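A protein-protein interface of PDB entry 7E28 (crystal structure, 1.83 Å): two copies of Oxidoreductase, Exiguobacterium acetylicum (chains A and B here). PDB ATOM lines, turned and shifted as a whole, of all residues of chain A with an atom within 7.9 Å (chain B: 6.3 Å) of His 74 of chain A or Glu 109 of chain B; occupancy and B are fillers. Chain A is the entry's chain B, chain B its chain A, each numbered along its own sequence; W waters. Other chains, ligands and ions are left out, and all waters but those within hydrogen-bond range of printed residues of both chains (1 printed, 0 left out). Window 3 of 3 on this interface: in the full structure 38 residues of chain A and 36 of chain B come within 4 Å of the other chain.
Of the 23 printed residues of chain A, 6 touch a printed residue of chain B. Printed residues of chain A that touch a printed residue of chain B: Asn 70, His 74, Glu 117, Thr 120, Ile 121 and Leu 125. Of the 12 printed residues of chain B, 4 touch a printed residue of chain A. Hydrophobic or aromatic side chains of chain B within 4 Å of the printed part of chain A: Leu 105 and Leu 112.
No position is printed for both chains. Of the 8 pairs that touch across the chains among the printed residues, none has its exchanged pair printed and touching as well.
His 74 of chain A touches just these residues of chain B: Leu 105 and Glu 109. Of the printed residues of chain A, Glu 109 of chain B touches His 74 (2.8 Å) and Ile 121 (3.4 Å). Of the printed residues of chain B, Glu 117 of chain A touches Leu 112. Of the printed residues of chain A, Leu 105 of chain B touches His 74 (3.5 Å), Ile 121 (3.9 Å) and Leu 125 (3.5 Å). The nearest printed residue of chain B that does not touch Leu 125 of chain A is Glu 109 of chain B (6.8 Å).
A ring nitrogen (NE2) of His 74 of chain A lies within hydrogen-bond range of the side-chain carboxylate (OE2) of Glu 109 of chain B, 2.8 Å away. The guanidinium group (NH2) of Arg 113 of chain B lies close to the side-chain amide nitrogen (ND2) of Asn 70 of chain A (3.4 Å).
Water W1 lies within hydrogen-bond range of OE1 of Glu 109 of chain B (2.9 Å), NE2 of His 74 of chain A (3.3 Å), O of Asn 70 of chain A (3.3 Å) and N of Gln 71 of chain A (3.5 Å).
Among the printed residues, pairs that only touch across the chains: His 74 of chain A with Leu 105 of chain B (3.5 Å), Glu 117 of chain A with Leu 112 of chain B (3.7 Å), Thr 120 of chain A with Leu 112 of chain B (3.9 Å), Ile 121 of chain A with Leu 105 of chain B (3.9 Å), Ile 121 of chain A with Glu 109 of chain B (3.4 Å) and Leu 125 of chain A with Leu 105 of chain B (3.5 Å).
The side-chain amide oxygen (OD1) of Asn 70 of chain A sits close to the side-chain carboxylate (OE2) of Glu 117 of chain A, 3.2 Å away. OH of Tyr 77 of chain A lies within hydrogen-bond range of O of Leu 125 of chain A, 3.1 Å away. O of Thr 120 of chain A lies within hydrogen-bond range of OG of Ser 124 of chain A (2.6 Å).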
ATOM      1  N   VAL A  65     -20.270 -12.941  11.369  1.00  0.00           N
ATOM      2  CA  VAL A  65     -20.283 -14.176  10.592  1.00  0.00           C
ATOM      3  C   VAL A  65     -21.042 -13.943   9.294  1.00  0.00           C
ATOM      4  O   VAL A  65     -22.004 -13.172   9.243  1.00  0.00           O
ATOM      5  CB  VAL A  65     -20.883 -15.336  11.427  1.00  0.00           C
ATOM      6  CG1 VAL A  65     -22.230 -14.941  11.925  1.00  0.00           C
ATOM      7  CG2 VAL A  65     -20.946 -16.635  10.638  1.00  0.00           C
ATOM      8  N   LEU A  67     -23.508 -15.569   7.198  1.00  0.00           N
ATOM      9  CA  LEU A  67     -24.464 -16.674   7.237  1.00  0.00           C
ATOM     10  C   LEU A  67     -24.797 -17.237   5.855  1.00  0.00           C
ATOM     11  O   LEU A  67     -25.668 -18.126   5.809  1.00  0.00           O
ATOM     12  CB  LEU A  67     -25.746 -16.223   7.940  1.00  0.00           C
ATOM     13  CG  LEU A  67     -25.589 -15.950   9.443  1.00  0.00           C
ATOM     14  CD1 LEU A  67     -26.844 -15.304  10.025  1.00  0.00           C
ATOM     15  CD2 LEU A  67     -25.223 -17.245  10.174  1.00  0.00           C
ATOM     16  N   ASP A  69     -22.708 -18.962   4.164  1.00  0.00           N
ATOM     17  CA  ASP A  69     -21.958 -20.209   4.109  1.00  0.00           C
ATOM     18  C   ASP A  69     -22.562 -21.196   5.111  1.00  0.00           C
ATOM     19  O   ASP A  69     -22.641 -20.897   6.309  1.00  0.00           O
ATOM     20  CB  ASP A  69     -20.477 -19.963   4.403  1.00  0.00           C
ATOM     21  CG  ASP A  69     -19.661 -21.233   4.360  1.00  0.00           C
ATOM     22  OD1 ASP A  69     -19.833 -22.076   5.264  1.00  0.00           O
ATOM     23  OD2 ASP A  69     -18.862 -21.408   3.413  1.00  0.00           O
ATOM     24  N   ASN A  70     -22.981 -22.367   4.612  1.00  0.00           N
ATOM     25  CA  ASN A  70     -23.721 -23.321   5.443  1.00  0.00           C
ATOM     26  C   ASN A  70     -22.913 -23.731   6.676  1.00  0.00           C
ATOM     27  O   ASN A  70     -23.465 -23.874   7.775  1.00  0.00           O
ATOM     28  CB  ASN A  70     -24.106 -24.560   4.618  1.00  0.00           C
ATOM     29  CG  ASN A  70     -25.330 -24.331   3.706  1.00  0.00           C
ATOM     30  OD1 ASN A  70     -25.982 -23.283   3.759  1.00  0.00           O
ATOM     31  ND2 ASN A  70     -25.627 -25.318   2.852  1.00  0.00           N
ATOM     32  N   GLN A  71     -21.600 -23.922   6.515  1.00  0.00           N
ATOM     33  CA  GLN A  71     -20.776 -24.321   7.649  1.00  0.00           C
ATOM     34  C   GLN A  71     -20.697 -23.212   8.694  1.00  0.00           C
ATOM     35  O   GLN A  71     -20.781 -23.478   9.901  1.00  0.00           O
ATOM     36  CB  GLN A  71     -19.381 -24.719   7.185  1.00  0.00           C
ATOM     37  CG  GLN A  71     -18.458 -25.142   8.323  1.00  0.00           C
ATOM     38  CD  GLN A  71     -18.981 -26.333   9.118  1.00  0.00           C
ATOM     39  OE1 GLN A  71     -19.192 -27.410   8.567  1.00  0.00           O
ATOM     40  NE2 GLN A  71     -19.182 -26.146  10.421  1.00  0.00           N
ATOM     41  N   ASN A  72     -20.527 -21.962   8.252  1.00  0.00           N
ATOM     42  CA  ASN A  72     -20.539 -20.833   9.180  1.00  0.00           C
ATOM     43  C   ASN A  72     -21.802 -20.820  10.025  1.00  0.00           C
ATOM     44  O   ASN A  72     -21.768 -20.466  11.210  1.00  0.00           O
ATOM     45  CB  ASN A  72     -20.416 -19.518   8.410  1.00  0.00           C
ATOM     46  CG  ASN A  72     -19.029 -19.299   7.867  1.00  0.00           C
ATOM     47  OD1 ASN A  72     -18.105 -20.051   8.186  1.00  0.00           O
ATOM     48  ND2 ASN A  72     -18.866 -18.265   7.039  1.00  0.00           N
ATOM     49  N   VAL A  73     -22.932 -21.199   9.424  1.00  0.00           N
ATOM     50  CA  VAL A  73     -24.195 -21.259  10.155  1.00  0.00           C
ATOM     51  C   VAL A  73     -24.108 -22.288  11.273  1.00  0.00           C
ATOM     52  O   VAL A  73     -24.561 -22.042  12.392  1.00  0.00           O
ATOM     53  CB  VAL A  73     -25.362 -21.579   9.200  1.00  0.00           C
ATOM     54  CG1 VAL A  73     -26.679 -21.625   9.965  1.00  0.00           C
ATOM     55  CG2 VAL A  73     -25.418 -20.553   8.024  1.00  0.00           C
ATOM     56  N   HIS A  74     -23.541 -23.460  10.982  1.00  0.00           N
ATOM     57  CA  HIS A  74     -23.359 -24.472  12.016  1.00  0.00           C
ATOM     58  C   HIS A  74     -22.459 -23.947  13.124  1.00  0.00           C
ATOM     59  O   HIS A  74     -22.792 -24.039  14.310  1.00  0.00           O
ATOM     60  CB  HIS A  74     -22.771 -25.753  11.414  1.00  0.00           C
ATOM     61  CG  HIS A  74     -23.773 -26.574  10.663  1.00  0.00           C
ATOM     62  ND1 HIS A  74     -24.645 -27.446  11.285  1.00  0.00           N
ATOM     63  CD2 HIS A  74     -24.074 -26.618   9.342  1.00  0.00           C
ATOM     64  CE1 HIS A  74     -25.428 -28.004  10.376  1.00  0.00           C
ATOM     65  NE2 HIS A  74     -25.102 -27.518   9.189  1.00  0.00           N
ATOM     66  N   ASP A  75     -21.302 -23.390  12.739  1.00  0.00           N
ATOM     67  CA  ASP A  75     -20.358 -22.852  13.717  1.00  0.00           C
ATOM     68  C   ASP A  75     -21.031 -21.834  14.622  1.00  0.00           C
ATOM     69  O   ASP A  75     -20.913 -21.907  15.851  1.00  0.00           O
ATOM     70  CB  ASP A  75     -19.164 -22.225  13.009  1.00  0.00           C
ATOM     71  CG  ASP A  75     -18.386 -23.226  12.220  1.00  0.00           C
ATOM     72  OD1 ASP A  75     -18.630 -24.433  12.433  1.00  0.00           O
ATOM     73  OD2 ASP A  75     -17.546 -22.811  11.383  1.00  0.00           O
ATOM     74  N   LEU A  76     -21.745 -20.870  14.032  1.00  0.00           N
ATOM     75  CA  LEU A  76     -22.521 -19.950  14.854  1.00  0.00           C
ATOM     76  C   LEU A  76     -23.353 -20.709  15.882  1.00  0.00           C
ATOM     77  O   LEU A  76     -23.275 -20.434  17.088  1.00  0.00           O
ATOM     78  CB  LEU A  76     -23.423 -19.084  13.984  1.00  0.00           C
ATOM     79  CG  LEU A  76     -24.352 -18.261  14.877  1.00  0.00           C
ATOM     80  CD1 LEU A  76     -23.566 -17.147  15.548  1.00  0.00           C
ATOM     81  CD2 LEU A  76     -25.515 -17.715  14.091  1.00  0.00           C
ATOM     82  N   TYR A  77     -24.147 -21.691  15.429  1.00  0.00           N
ATOM     83  CA  TYR A  77     -25.043 -22.360  16.370  1.00  0.00           C
ATOM     84  C   TYR A  77     -24.267 -23.147  17.430  1.00  0.00           C
ATOM     85  O   TYR A  77     -24.635 -23.129  18.609  1.00  0.00           O
ATOM     86  CB  TYR A  77     -26.041 -23.272  15.651  1.00  0.00           C
ATOM     87  CG  TYR A  77     -27.073 -23.806  16.634  1.00  0.00           C
ATOM     88  CD1 TYR A  77     -28.220 -23.077  16.918  1.00  0.00           C
ATOM     89  CD2 TYR A  77     -26.851 -24.990  17.350  1.00  0.00           C
ATOM     90  CE1 TYR A  77     -29.142 -23.524  17.842  1.00  0.00           C
ATOM     91  CE2 TYR A  77     -27.776 -25.458  18.291  1.00  0.00           C
ATOM     92  CZ  TYR A  77     -28.913 -24.711  18.526  1.00  0.00           C
ATOM     93  OH  TYR A  77     -29.841 -25.143  19.437  1.00  0.00           O
ATOM     94  N   GLU A  78     -23.218 -23.875  17.027  1.00  0.00           N
ATOM     95  CA  GLU A  78     -22.400 -24.596  18.002  1.00  0.00           C
ATOM     96  C   GLU A  78     -21.838 -23.651  19.048  1.00  0.00           C
ATOM     97  O   GLU A  78     -21.852 -23.950  20.249  1.00  0.00           O
ATOM     98  CB  GLU A  78     -21.263 -25.350  17.309  1.00  0.00           C
ATOM     99  CG  GLU A  78     -21.719 -26.553  16.508  1.00  0.00           C
ATOM    100  CD  GLU A  78     -22.581 -27.538  17.311  1.00  0.00           C
ATOM    101  OE1 GLU A  78     -23.821 -27.365  17.376  1.00  0.00           O
ATOM    102  OE2 GLU A  78     -22.033 -28.526  17.840  1.00  0.00           O
ATOM    103  N   GLY A  79     -21.345 -22.498  18.606  1.00  0.00           N
ATOM    104  CA  GLY A  79     -20.723 -21.576  19.532  1.00  0.00           C
ATOM    105  C   GLY A  79     -21.681 -21.020  20.563  1.00  0.00           C
ATOM    106  O   GLY A  79     -21.254 -20.551  21.620  1.00  0.00           O
ATOM    107  N   LEU A  80     -22.984 -21.046  20.272  1.00  0.00           N
ATOM    108  CA  LEU A  80     -23.987 -20.607  21.235  1.00  0.00           C
ATOM    109  C   LEU A  80     -24.709 -21.756  21.917  1.00  0.00           C
ATOM    110  O   LEU A  80     -25.412 -21.517  22.904  1.00  0.00           O
ATOM    111  CB  LEU A  80     -25.034 -19.717  20.553  1.00  0.00           C
ATOM    112  CG  LEU A  80     -24.584 -18.576  19.638  1.00  0.00           C
ATOM    113  CD1 LEU A  80     -25.797 -17.977  18.965  1.00  0.00           C
ATOM    114  CD2 LEU A  80     -23.830 -17.495  20.406  1.00  0.00           C
ATOM    115  N   LYS A  81     -24.542 -22.979  21.406  1.00  0.00           N
ATOM    116  CA  LYS A  81     -25.249 -24.195  21.804  1.00  0.00           C
ATOM    117  C   LYS A  81     -25.637 -24.218  23.281  1.00  0.00           C
ATOM    118  O   LYS A  81     -26.825 -24.312  23.603  1.00  0.00           O
ATOM    119  CB  LYS A  81     -24.383 -25.421  21.470  1.00  0.00           C
ATOM    120  CG  LYS A  81     -25.121 -26.691  21.070  1.00  0.00           C
ATOM    121  CD  LYS A  81     -24.089 -27.767  20.737  1.00  0.00           C
ATOM    122  CE  LYS A  81     -24.703 -29.055  20.204  1.00  0.00           C
ATOM    123  NZ  LYS A  81     -25.908 -29.502  20.960  1.00  0.00           N
ATOM    124  N   GLU A 117     -31.511 -21.133   3.349  1.00  0.00           N
ATOM    125  CA  GLU A 117     -30.640 -22.128   3.974  1.00  0.00           C
ATOM    126  C   GLU A 117     -30.286 -21.755   5.415  1.00  0.00           C
ATOM    127  O   GLU A 117     -30.489 -22.555   6.343  1.00  0.00           O
ATOM    128  CB  GLU A 117     -29.396 -22.326   3.112  1.00  0.00           C
ATOM    129  CG  GLU A 117     -29.718 -23.321   2.010  1.00  0.00           C
ATOM    130  CD  GLU A 117     -28.790 -23.294   0.828  1.00  0.00           C
ATOM    131  OE1 GLU A 117     -29.300 -23.626  -0.259  1.00  0.00           O
ATOM    132  OE2 GLU A 117     -27.589 -22.989   0.976  1.00  0.00           O
ATOM    133  N   ALA A 118     -29.755 -20.549   5.630  1.00  0.00           N
ATOM    134  CA  ALA A 118     -29.438 -20.135   6.995  1.00  0.00           C
ATOM    135  C   ALA A 118     -30.668 -20.239   7.879  1.00  0.00           C
ATOM    136  O   ALA A 118     -30.604 -20.780   8.990  1.00  0.00           O
ATOM    137  CB  ALA A 118     -28.884 -18.715   7.008  1.00  0.00           C
ATOM    138  N   THR A 120     -33.248 -22.140   7.553  1.00  0.00           N
ATOM    139  CA  THR A 120     -33.685 -23.517   7.761  1.00  0.00           C
ATOM    140  C   THR A 120     -32.763 -24.244   8.735  1.00  0.00           C
ATOM    141  O   THR A 120     -33.223 -25.016   9.590  1.00  0.00           O
ATOM    142  CB  THR A 120     -33.748 -24.256   6.419  1.00  0.00           C
ATOM    143  OG1 THR A 120     -34.734 -23.635   5.592  1.00  0.00           O
ATOM    144  CG2 THR A 120     -34.133 -25.700   6.617  1.00  0.00           C
ATOM    145  N   ILE A 121     -31.452 -24.040   8.593  1.00  0.00           N
ATOM    146  CA  ILE A 121     -30.494 -24.733   9.449  1.00  0.00           C
ATOM    147  C   ILE A 121     -30.661 -24.276  10.889  1.00  0.00           C
ATOM    148  O   ILE A 121     -30.775 -25.094  11.815  1.00  0.00           O
ATOM    149  CB  ILE A 121     -29.058 -24.494   8.948  1.00  0.00           C
ATOM    150  CG1 ILE A 121     -28.870 -25.086   7.531  1.00  0.00           C
ATOM    151  CG2 ILE A 121     -28.049 -25.035   9.933  1.00  0.00           C
ATOM    152  CD1 ILE A 121     -27.639 -24.586   6.817  1.00  0.00           C
ATOM    153  N   LEU A 122     -30.694 -22.960  11.094  1.00  0.00           N
ATOM    154  CA  LEU A 122     -30.822 -22.423  12.438  1.00  0.00           C
ATOM    155  C   LEU A 122     -32.168 -22.780  13.054  1.00  0.00           C
ATOM    156  O   LEU A 122     -32.231 -23.174  14.225  1.00  0.00           O
ATOM    157  CB  LEU A 122     -30.610 -20.915  12.414  1.00  0.00           C
ATOM    158  CG  LEU A 122     -29.153 -20.543  12.139  1.00  0.00           C
ATOM    159  CD1 LEU A 122     -29.024 -19.041  11.875  1.00  0.00           C
ATOM    160  CD2 LEU A 122     -28.205 -21.020  13.258  1.00  0.00           C
ATOM    161  N   SER A 124     -33.910 -25.441  12.340  1.00  0.00           N
ATOM    162  CA  SER A 124     -33.823 -26.863  12.660  1.00  0.00           C
ATOM    163  C   SER A 124     -33.025 -27.093  13.937  1.00  0.00           C
ATOM    164  O   SER A 124     -33.448 -27.859  14.810  1.00  0.00           O
ATOM    165  CB  SER A 124     -33.201 -27.626  11.494  1.00  0.00           C
ATOM    166  OG  SER A 124     -33.986 -27.445  10.318  1.00  0.00           O
ATOM    167  N   LEU A 125     -31.866 -26.433  14.066  1.00  0.00           N
ATOM    168  CA  LEU A 125     -31.028 -26.658  15.240  1.00  0.00           C
ATOM    169  C   LEU A 125     -31.701 -26.127  16.494  1.00  0.00           C
ATOM    170  O   LEU A 125     -31.669 -26.778  17.546  1.00  0.00           O
ATOM    171  CB  LEU A 125     -29.654 -26.014  15.054  1.00  0.00           C
ATOM    172  CG  LEU A 125     -28.786 -26.705  13.996  1.00  0.00           C
ATOM    173  CD1 LEU A 125     -27.504 -25.936  13.762  1.00  0.00           C
ATOM    174  CD2 LEU A 125     -28.503 -28.152  14.349  1.00  0.00           C
ATOM    175  N   ARG A 128     -34.525 -28.535  17.475  1.00  0.00           N
ATOM    176  CA  ARG A 128     -34.001 -29.797  17.989  1.00  0.00           C
ATOM    177  C   ARG A 128     -33.734 -29.716  19.490  1.00  0.00           C
ATOM    178  O   ARG A 128     -34.152 -30.590  20.259  1.00  0.00           O
ATOM    179  CB  ARG A 128     -32.722 -30.167  17.225  1.00  0.00           C
ATOM    180  CG  ARG A 128     -32.118 -31.517  17.593  1.00  0.00           C
ATOM    181  CD  ARG A 128     -30.677 -31.654  17.079  1.00  0.00           C
ATOM    182  NE  ARG A 128     -29.807 -30.615  17.632  1.00  0.00           N
ATOM    183  CZ  ARG A 128     -28.534 -30.415  17.275  1.00  0.00           C
ATOM    184  NH1 ARG A 128     -27.963 -31.191  16.346  1.00  0.00           N
ATOM    185  NH2 ARG A 128     -27.829 -29.438  17.847  1.00  0.00           N
ATOM    186  N   PHE B  94     -35.550 -34.486  -4.225  1.00  0.00           N
ATOM    187  CA  PHE B  94     -36.015 -35.578  -3.389  1.00  0.00           C
ATOM    188  C   PHE B  94     -36.687 -34.985  -2.158  1.00  0.00           C
ATOM    189  O   PHE B  94     -36.685 -33.768  -1.942  1.00  0.00           O
ATOM    190  CB  PHE B  94     -34.867 -36.508  -3.001  1.00  0.00           C
ATOM    191  CG  PHE B  94     -33.797 -35.837  -2.200  1.00  0.00           C
ATOM    192  CD1 PHE B  94     -32.681 -35.297  -2.831  1.00  0.00           C
ATOM    193  CD2 PHE B  94     -33.898 -35.750  -0.813  1.00  0.00           C
ATOM    194  CE1 PHE B  94     -31.680 -34.682  -2.089  1.00  0.00           C
ATOM    195  CE2 PHE B  94     -32.904 -35.136  -0.067  1.00  0.00           C
ATOM    196  CZ  PHE B  94     -31.792 -34.600  -0.703  1.00  0.00           C
ATOM    197  N   GLU B 104     -32.274 -34.876   9.739  1.00  0.00           N
ATOM    198  CA  GLU B 104     -30.847 -35.016   9.452  1.00  0.00           C
ATOM    199  C   GLU B 104     -30.418 -33.832   8.573  1.00  0.00           C
ATOM    200  O   GLU B 104     -30.845 -33.727   7.414  1.00  0.00           O
ATOM    201  CB  GLU B 104     -30.611 -36.362   8.769  1.00  0.00           C
ATOM    202  CG  GLU B 104     -29.186 -36.683   8.345  1.00  0.00           C
ATOM    203  CD  GLU B 104     -29.160 -37.808   7.322  1.00  0.00           C
ATOM    204  OE1 GLU B 104     -29.948 -38.765   7.501  1.00  0.00           O
ATOM    205  OE2 GLU B 104     -28.373 -37.733   6.346  1.00  0.00           O
ATOM    206  N   LEU B 105     -29.572 -32.934   9.113  1.00  0.00           N
ATOM    207  CA  LEU B 105     -29.312 -31.669   8.415  1.00  0.00           C
ATOM    208  C   LEU B 105     -28.495 -31.850   7.137  1.00  0.00           C
ATOM    209  O   LEU B 105     -28.636 -31.050   6.202  1.00  0.00           O
ATOM    210  CB  LEU B 105     -28.626 -30.662   9.339  1.00  0.00           C
ATOM    211  CG  LEU B 105     -29.589 -29.643   9.971  1.00  0.00           C
ATOM    212  CD1 LEU B 105     -28.858 -28.688  10.866  1.00  0.00           C
ATOM    213  CD2 LEU B 105     -30.397 -28.882   8.910  1.00  0.00           C
ATOM    214  N   GLY B 106     -27.634 -32.867   7.070  1.00  0.00           N
ATOM    215  CA  GLY B 106     -26.910 -33.115   5.833  1.00  0.00           C
ATOM    216  C   GLY B 106     -27.841 -33.428   4.674  1.00  0.00           C
ATOM    217  O   GLY B 106     -27.656 -32.939   3.555  1.00  0.00           O
ATOM    218  N   LYS B 107     -28.872 -34.237   4.934  1.00  0.00           N
ATOM    219  CA  LYS B 107     -29.882 -34.508   3.917  1.00  0.00           C
ATOM    220  C   LYS B 107     -30.655 -33.246   3.555  1.00  0.00           C
ATOM    221  O   LYS B 107     -30.779 -32.896   2.373  1.00  0.00           O
ATOM    222  CB  LYS B 107     -30.837 -35.596   4.397  1.00  0.00           C
ATOM    223  CG  LYS B 107     -31.944 -35.916   3.420  1.00  0.00           C
ATOM    224  CD  LYS B 107     -32.818 -37.049   3.941  1.00  0.00           C
ATOM    225  CE  LYS B 107     -33.807 -37.539   2.892  1.00  0.00           C
ATOM    226  NZ  LYS B 107     -34.834 -38.482   3.463  1.00  0.00           N
ATOM    227  N   ILE B 108     -31.183 -32.544   4.559  1.00  0.00           N
ATOM    228  CA  ILE B 108     -32.041 -31.406   4.244  1.00  0.00           C
ATOM    229  C   ILE B 108     -31.261 -30.317   3.506  1.00  0.00           C
ATOM    230  O   ILE B 108     -31.804 -29.644   2.614  1.00  0.00           O
ATOM    231  CB  ILE B 108     -32.724 -30.879   5.523  1.00  0.00           C
ATOM    232  CG1 ILE B 108     -34.070 -31.604   5.790  1.00  0.00           C
ATOM    233  CG2 ILE B 108     -32.899 -29.365   5.460  1.00  0.00           C
ATOM    234  CD1 ILE B 108     -34.038 -33.126   5.645  1.00  0.00           C
ATOM    235  N   GLU B 109     -29.972 -30.153   3.824  1.00  0.00           N
ATOM    236  CA  GLU B 109     -29.165 -29.173   3.108  1.00  0.00           C
ATOM    237  C   GLU B 109     -28.980 -29.585   1.646  1.00  0.00           C
ATOM    238  O   GLU B 109     -29.170 -28.773   0.727  1.00  0.00           O
ATOM    239  CB  GLU B 109     -27.831 -28.983   3.837  1.00  0.00           C
ATOM    240  CG  GLU B 109     -28.001 -28.148   5.102  1.00  0.00           C
ATOM    241  CD  GLU B 109     -26.834 -28.237   6.070  1.00  0.00           C
ATOM    242  OE1 GLU B 109     -25.696 -28.530   5.638  1.00  0.00           O
ATOM    243  OE2 GLU B 109     -27.058 -27.979   7.270  1.00  0.00           O
ATOM    244  N   LYS B 110     -28.663 -30.862   1.409  1.00  0.00           N
ATOM    245  CA  LYS B 110     -28.636 -31.373   0.044  1.00  0.00           C
ATOM    246  C   LYS B 110     -29.965 -31.113  -0.662  1.00  0.00           C
ATOM    247  O   LYS B 110     -29.987 -30.667  -1.825  1.00  0.00           O
ATOM    248  CB  LYS B 110     -28.310 -32.868   0.043  1.00  0.00           C
ATOM    249  CG  LYS B 110     -28.038 -33.442  -1.354  1.00  0.00           C
ATOM    250  CD  LYS B 110     -27.328 -34.789  -1.302  1.00  0.00           C
ATOM    251  CE  LYS B 110     -27.465 -35.542  -2.616  1.00  0.00           C
ATOM    252  NZ  LYS B 110     -27.246 -37.014  -2.480  1.00  0.00           N
ATOM    253  N   MET B 111     -31.079 -31.355   0.041  1.00  0.00           N
ATOM    254  CA  MET B 111     -32.400 -31.157  -0.551  1.00  0.00           C
ATOM    255  C   MET B 111     -32.605 -29.708  -0.975  1.00  0.00           C
ATOM    256  O   MET B 111     -33.069 -29.436  -2.097  1.00  0.00           O
ATOM    257  CB  MET B 111     -33.491 -31.580   0.429  1.00  0.00           C
ATOM    258  CG  MET B 111     -34.907 -31.453  -0.136  1.00  0.00           C
ATOM    259  SD  MET B 111     -36.130 -31.945   1.108  1.00  0.00           S
ATOM    260  CE  MET B 111     -36.325 -30.412   1.967  1.00  0.00           C
ATOM    261  N   LEU B 112     -32.246 -28.762  -0.104  1.00  0.00           N
ATOM    262  CA  LEU B 112     -32.345 -27.348  -0.462  1.00  0.00           C
ATOM    263  C   LEU B 112     -31.492 -27.018  -1.685  1.00  0.00           C
ATOM    264  O   LEU B 112     -31.889 -26.204  -2.531  1.00  0.00           O
ATOM    265  CB  LEU B 112     -31.928 -26.477   0.728  1.00  0.00           C
ATOM    266  CG  LEU B 112     -32.836 -26.636   1.959  1.00  0.00           C
ATOM    267  CD1 LEU B 112     -32.299 -25.769   3.081  1.00  0.00           C
ATOM    268  CD2 LEU B 112     -34.297 -26.300   1.684  1.00  0.00           C
ATOM    269  N   ARG B 113     -30.317 -27.639  -1.796  1.00  0.00           N
ATOM    270  CA  ARG B 113     -29.428 -27.322  -2.909  1.00  0.00           C
ATOM    271  C   ARG B 113     -29.974 -27.881  -4.213  1.00  0.00           C
ATOM    272  O   ARG B 113     -29.731 -27.318  -5.288  1.00  0.00           O
ATOM    273  CB  ARG B 113     -28.033 -27.875  -2.641  1.00  0.00           C
ATOM    274  CG  ARG B 113     -27.263 -27.120  -1.573  1.00  0.00           C
ATOM    275  CD  ARG B 113     -25.823 -27.594  -1.518  1.00  0.00           C
ATOM    276  NE  ARG B 113     -25.237 -27.469  -0.191  1.00  0.00           N
ATOM    277  CZ  ARG B 113     -24.807 -28.495   0.540  1.00  0.00           C
ATOM    278  NH1 ARG B 113     -24.896 -29.739   0.072  1.00  0.00           N
ATOM    279  NH2 ARG B 113     -24.281 -28.269   1.736  1.00  0.00           N
ATOM    280  N   LEU B 114     -30.696 -29.000  -4.136  1.00  0.00           N
ATOM    281  CA  LEU B 114     -31.219 -29.650  -5.333  1.00  0.00           C
ATOM    282  C   LEU B 114     -32.577 -29.081  -5.714  1.00  0.00           C
ATOM    283  O   LEU B 114     -32.754 -28.551  -6.818  1.00  0.00           O
ATOM    284  CB  LEU B 114     -31.326 -31.156  -5.108  1.00  0.00           C
ATOM    285  CG  LEU B 114     -30.182 -32.042  -5.575  1.00  0.00           C
ATOM    286  CD1 LEU B 114     -30.607 -33.491  -5.491  1.00  0.00           C
ATOM    287  CD2 LEU B 114     -29.791 -31.699  -7.006  1.00  0.00           C
HETATM  288  O   HOH W   1     -23.472 -26.872   6.442  1.00  0.00           O
